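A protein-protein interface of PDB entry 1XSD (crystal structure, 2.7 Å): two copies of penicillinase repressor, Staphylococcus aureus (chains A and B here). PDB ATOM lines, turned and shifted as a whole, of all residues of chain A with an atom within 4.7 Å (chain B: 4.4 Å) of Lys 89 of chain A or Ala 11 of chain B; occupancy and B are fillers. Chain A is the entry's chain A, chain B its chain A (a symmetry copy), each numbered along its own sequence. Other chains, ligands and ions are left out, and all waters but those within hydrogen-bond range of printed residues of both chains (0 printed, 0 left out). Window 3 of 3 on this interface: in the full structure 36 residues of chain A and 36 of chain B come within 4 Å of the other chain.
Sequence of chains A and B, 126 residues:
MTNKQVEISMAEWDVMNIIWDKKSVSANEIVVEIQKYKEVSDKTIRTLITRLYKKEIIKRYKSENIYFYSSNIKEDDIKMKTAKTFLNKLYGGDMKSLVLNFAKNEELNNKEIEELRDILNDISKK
O of Trp 13 of chain B lies within hydrogen-bond range of ND2 of Asn 17 of chain B (3.3 Å).
No position is printed for both chains.
Of the printed residues of chain B, Leu 90 of chain A touches Trp 13.
Of the printed residues of chain A, Met 10 of chain B touches Lys 89.
Of the printed residues of chain A, Trp 13 of chain B touches Leu 90.
Of the printed residues of chain A, Asp 14 of chain B touches Lys 89 (3.2 Å).
The nearest residue of chain B that does not touch Lys 89 of chain A is Trp 13 of chain B (4.2 Å).
The nearest printed residue of chain A that does not touch Ala 11 of chain B is Thr 85 of chain A (8.7 Å).
Of the 7 printed residues of chain A, 2 touch a printed residue of chain B.
Hydrophobic or aromatic side chains of chain A within 4 Å of the printed part of chain B: Leu 90.
Hydrophobic or aromatic side chains of chain B that line the printed part of chain A: Trp 13.
Along chain B the printed residues that touch a printed residue of chain A span positions 10 to 17.
Among the printed residues, merely in contact across the chains: Lys 89 of chain A with Ala 11 of chain B (3.6 Å) and Leu 90 of chain A with Trp 13 of chain B (3.6 Å).
O of Met 10 of chain B is in hydrogen-bond range of NZ of Lys 89 of chain A (2.7 Å).
NZ of Lys 89 of chain A is in salt-bridge range of OD2 of Asp 14 of chain B (3.2 Å).
The backbone carbonyl oxygen (O) of Lys 89 of chain A is in hydrogen-bond range of the side-chain amide nitrogen (ND2) of Asn 17 of chain B (2.8 Å).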
ATOM      1  N   THR A  85      -6.263  -8.102  21.564  1.00  0.00           N
ATOM      2  CA  THR A  85      -4.887  -7.950  21.957  1.00  0.00           C
ATOM      3  C   THR A  85      -4.220  -9.281  22.088  1.00  0.00           C
ATOM      4  O   THR A  85      -3.099  -9.495  21.587  1.00  0.00           O
ATOM      5  CB  THR A  85      -4.786  -7.216  23.245  1.00  0.00           C
ATOM      6  OG1 THR A  85      -4.890  -5.828  22.941  1.00  0.00           O
ATOM      7  CG2 THR A  85      -3.414  -7.478  23.927  1.00  0.00           C
ATOM      8  N   PHE A  86      -4.927 -10.161  22.783  1.00  0.00           N
ATOM      9  CA  PHE A  86      -4.491 -11.514  23.015  1.00  0.00           C
ATOM     10  C   PHE A  86      -4.315 -12.261  21.688  1.00  0.00           C
ATOM     11  O   PHE A  86      -3.249 -12.823  21.417  1.00  0.00           O
ATOM     12  CB  PHE A  86      -5.533 -12.186  23.871  1.00  0.00           C
ATOM     13  CG  PHE A  86      -5.564 -13.639  23.726  1.00  0.00           C
ATOM     14  CD1 PHE A  86      -4.648 -14.429  24.402  1.00  0.00           C
ATOM     15  CD2 PHE A  86      -6.512 -14.233  22.911  1.00  0.00           C
ATOM     16  CE1 PHE A  86      -4.668 -15.831  24.276  1.00  0.00           C
ATOM     17  CE2 PHE A  86      -6.561 -15.615  22.762  1.00  0.00           C
ATOM     18  CZ  PHE A  86      -5.633 -16.428  23.450  1.00  0.00           C
ATOM     19  N   LEU A  87      -5.359 -12.262  20.863  1.00  0.00           N
ATOM     20  CA  LEU A  87      -5.320 -12.939  19.573  1.00  0.00           C
ATOM     21  C   LEU A  87      -4.165 -12.426  18.638  1.00  0.00           C
ATOM     22  O   LEU A  87      -3.517 -13.187  17.915  1.00  0.00           O
ATOM     23  CB  LEU A  87      -6.684 -12.762  18.915  1.00  0.00           C
ATOM     24  CG  LEU A  87      -7.320 -14.016  18.316  1.00  0.00           C
ATOM     25  CD1 LEU A  87      -6.392 -14.526  17.265  1.00  0.00           C
ATOM     26  CD2 LEU A  87      -7.585 -15.081  19.359  1.00  0.00           C
ATOM     27  N   ASN A  88      -3.911 -11.129  18.657  1.00  0.00           N
ATOM     28  CA  ASN A  88      -2.845 -10.577  17.837  1.00  0.00           C
ATOM     29  C   ASN A  88      -1.461 -11.073  18.284  1.00  0.00           C
ATOM     30  O   ASN A  88      -0.566 -11.424  17.468  1.00  0.00           O
ATOM     31  CB  ASN A  88      -2.884  -9.062  17.937  1.00  0.00           C
ATOM     32  CG  ASN A  88      -4.058  -8.491  17.228  1.00  0.00           C
ATOM     33  OD1 ASN A  88      -4.624  -9.137  16.340  1.00  0.00           O
ATOM     34  ND2 ASN A  88      -4.432  -7.265  17.583  1.00  0.00           N
ATOM     35  N   LYS A  89      -1.289 -11.063  19.593  1.00  0.00           N
ATOM     36  CA  LYS A  89      -0.071 -11.505  20.175  1.00  0.00           C
ATOM     37  C   LYS A  89       0.087 -13.011  20.043  1.00  0.00           C
ATOM     38  O   LYS A  89       1.151 -13.464  19.675  1.00  0.00           O
ATOM     39  CB  LYS A  89      -0.024 -11.078  21.638  1.00  0.00           C
ATOM     40  CG  LYS A  89       0.191  -9.587  21.792  1.00  0.00           C
ATOM     41  CD  LYS A  89       1.510  -9.232  22.507  1.00  0.00           C
ATOM     42  CE  LYS A  89       2.000  -7.801  22.137  1.00  0.00           C
ATOM     43  NZ  LYS A  89       3.269  -7.397  22.842  1.00  0.00           N
ATOM     44  N   LEU A  90      -0.936 -13.815  20.300  1.00  0.00           N
ATOM     45  CA  LEU A  90      -0.699 -15.252  20.189  1.00  0.00           C
ATOM     46  C   LEU A  90      -1.044 -15.899  18.869  1.00  0.00           C
ATOM     47  O   LEU A  90      -0.624 -17.048  18.625  1.00  0.00           O
ATOM     48  CB  LEU A  90      -1.393 -16.022  21.315  1.00  0.00           C
ATOM     49  CG  LEU A  90      -0.605 -16.068  22.631  1.00  0.00           C
ATOM     50  CD1 LEU A  90      -0.175 -14.674  23.067  1.00  0.00           C
ATOM     51  CD2 LEU A  90      -1.462 -16.673  23.709  1.00  0.00           C
ATOM     52  N   TYR A  91      -1.775 -15.200  17.999  1.00  0.00           N
ATOM     53  CA  TYR A  91      -2.150 -15.819  16.724  1.00  0.00           C
ATOM     54  C   TYR A  91      -2.267 -14.865  15.546  1.00  0.00           C
ATOM     55  O   TYR A  91      -2.923 -15.205  14.563  1.00  0.00           O
ATOM     56  CB  TYR A  91      -3.478 -16.553  16.885  1.00  0.00           C
ATOM     57  CG  TYR A  91      -3.537 -17.511  18.066  1.00  0.00           C
ATOM     58  CD1 TYR A  91      -3.117 -18.842  17.946  1.00  0.00           C
ATOM     59  CD2 TYR A  91      -4.003 -17.090  19.298  1.00  0.00           C
ATOM     60  CE1 TYR A  91      -3.161 -19.730  19.037  1.00  0.00           C
ATOM     61  CE2 TYR A  91      -4.051 -17.955  20.395  1.00  0.00           C
ATOM     62  CZ  TYR A  91      -3.623 -19.271  20.266  1.00  0.00           C
ATOM     63  OH  TYR A  91      -3.584 -20.088  21.384  1.00  0.00           O
ATOM     64  N   SER B   9       6.203 -12.267  29.301  1.00  0.00           N
ATOM     65  CA  SER B   9       5.567 -10.986  29.483  1.00  0.00           C
ATOM     66  C   SER B   9       4.828 -10.618  28.177  1.00  0.00           C
ATOM     67  O   SER B   9       5.157 -11.110  27.114  1.00  0.00           O
ATOM     68  CB  SER B   9       6.624  -9.947  29.854  1.00  0.00           C
ATOM     69  OG  SER B   9       7.350  -9.510  28.719  1.00  0.00           O
ATOM     70  N   MET B  10       3.827  -9.749  28.270  1.00  0.00           N
ATOM     71  CA  MET B  10       3.052  -9.388  27.109  1.00  0.00           C
ATOM     72  C   MET B  10       3.946  -8.865  25.984  1.00  0.00           C
ATOM     73  O   MET B  10       3.743  -9.168  24.797  1.00  0.00           O
ATOM     74  CB  MET B  10       1.953  -8.363  27.514  1.00  0.00           C
ATOM     75  CG  MET B  10       0.651  -8.355  26.631  1.00  0.00           C
ATOM     76  SD  MET B  10      -0.084 -10.047  26.336  1.00  0.00           S
ATOM     77  CE  MET B  10      -0.017 -10.879  27.941  1.00  0.00           C
ATOM     78  N   ALA B  11       4.963  -8.110  26.352  1.00  0.00           N
ATOM     79  CA  ALA B  11       5.827  -7.541  25.339  1.00  0.00           C
ATOM     80  C   ALA B  11       6.845  -8.514  24.802  1.00  0.00           C
ATOM     81  O   ALA B  11       7.480  -8.243  23.781  1.00  0.00           O
ATOM     82  CB  ALA B  11       6.528  -6.322  25.895  1.00  0.00           C
ATOM     83  N   GLU B  12       6.990  -9.646  25.479  1.00  0.00           N
ATOM     84  CA  GLU B  12       7.953 -10.648  25.092  1.00  0.00           C
ATOM     85  C   GLU B  12       7.515 -11.515  23.918  1.00  0.00           C
ATOM     86  O   GLU B  12       8.370 -12.022  23.133  1.00  0.00           O
ATOM     87  CB  GLU B  12       8.265 -11.513  26.295  1.00  0.00           C
ATOM     88  CG  GLU B  12       9.538 -11.093  26.945  1.00  0.00           C
ATOM     89  CD  GLU B  12       9.616 -11.499  28.397  1.00  0.00           C
ATOM     90  OE1 GLU B  12       9.095 -12.601  28.718  1.00  0.00           O
ATOM     91  OE2 GLU B  12      10.203 -10.704  29.204  1.00  0.00           O
ATOM     92  N   TRP B  13       6.200 -11.694  23.792  1.00  0.00           N
ATOM     93  CA  TRP B  13       5.676 -12.495  22.723  1.00  0.00           C
ATOM     94  C   TRP B  13       6.208 -11.972  21.412  1.00  0.00           C
ATOM     95  O   TRP B  13       6.466 -12.739  20.504  1.00  0.00           O
ATOM     96  CB  TRP B  13       4.131 -12.467  22.719  1.00  0.00           C
ATOM     97  CG  TRP B  13       3.481 -13.185  23.917  1.00  0.00           C
ATOM     98  CD1 TRP B  13       3.056 -12.615  25.093  1.00  0.00           C
ATOM     99  CD2 TRP B  13       3.266 -14.595  24.062  1.00  0.00           C
ATOM    100  NE1 TRP B  13       2.598 -13.585  25.958  1.00  0.00           N
ATOM    101  CE2 TRP B  13       2.708 -14.808  25.350  1.00  0.00           C
ATOM    102  CE3 TRP B  13       3.497 -15.699  23.235  1.00  0.00           C
ATOM    103  CZ2 TRP B  13       2.367 -16.092  25.825  1.00  0.00           C
ATOM    104  CZ3 TRP B  13       3.161 -16.986  23.700  1.00  0.00           C
ATOM    105  CH2 TRP B  13       2.599 -17.170  24.984  1.00  0.00           C
ATOM    106  N   ASP B  14       6.400 -10.665  21.278  1.00  0.00           N
ATOM    107  CA  ASP B  14       6.883 -10.187  19.976  1.00  0.00           C
ATOM    108  C   ASP B  14       8.232 -10.775  19.642  1.00  0.00           C
ATOM    109  O   ASP B  14       8.551 -11.004  18.477  1.00  0.00           O
ATOM    110  CB  ASP B  14       6.973  -8.652  19.884  1.00  0.00           C
ATOM    111  CG  ASP B  14       5.650  -7.979  20.198  1.00  0.00           C
ATOM    112  OD1 ASP B  14       4.600  -8.561  19.833  1.00  0.00           O
ATOM    113  OD2 ASP B  14       5.671  -6.869  20.805  1.00  0.00           O
ATOM    114  N   ASN B  17       7.575 -14.794  19.073  1.00  0.00           N
ATOM    115  CA  ASN B  17       6.968 -15.125  17.812  1.00  0.00           C
ATOM    116  C   ASN B  17       8.009 -15.054  16.729  1.00  0.00           C
ATOM    117  O   ASN B  17       7.977 -15.834  15.782  1.00  0.00           O
ATOM    118  CB  ASN B  17       5.788 -14.231  17.511  1.00  0.00           C
ATOM    119  CG  ASN B  17       4.568 -14.645  18.281  1.00  0.00           C
ATOM    120  OD1 ASN B  17       4.272 -15.830  18.400  1.00  0.00           O
ATOM    121  ND2 ASN B  17       3.848 -13.673  18.804  1.00  0.00           N
ATOM    122  N   LEU B  48      14.517  -7.780  26.486  1.00  0.00           N
ATOM    123  CA  LEU B  48      13.505  -8.836  26.397  1.00  0.00           C
ATOM    124  C   LEU B  48      14.186 -10.171  26.088  1.00  0.00           C
ATOM    125  O   LEU B  48      13.926 -11.210  26.739  1.00  0.00           O
ATOM    126  CB  LEU B  48      12.490  -8.480  25.313  1.00  0.00           C
ATOM    127  CG  LEU B  48      11.750  -7.194  25.673  1.00  0.00           C
ATOM    128  CD1 LEU B  48      10.690  -6.851  24.625  1.00  0.00           C
ATOM    129  CD2 LEU B  48      11.127  -7.398  27.040  1.00  0.00           C
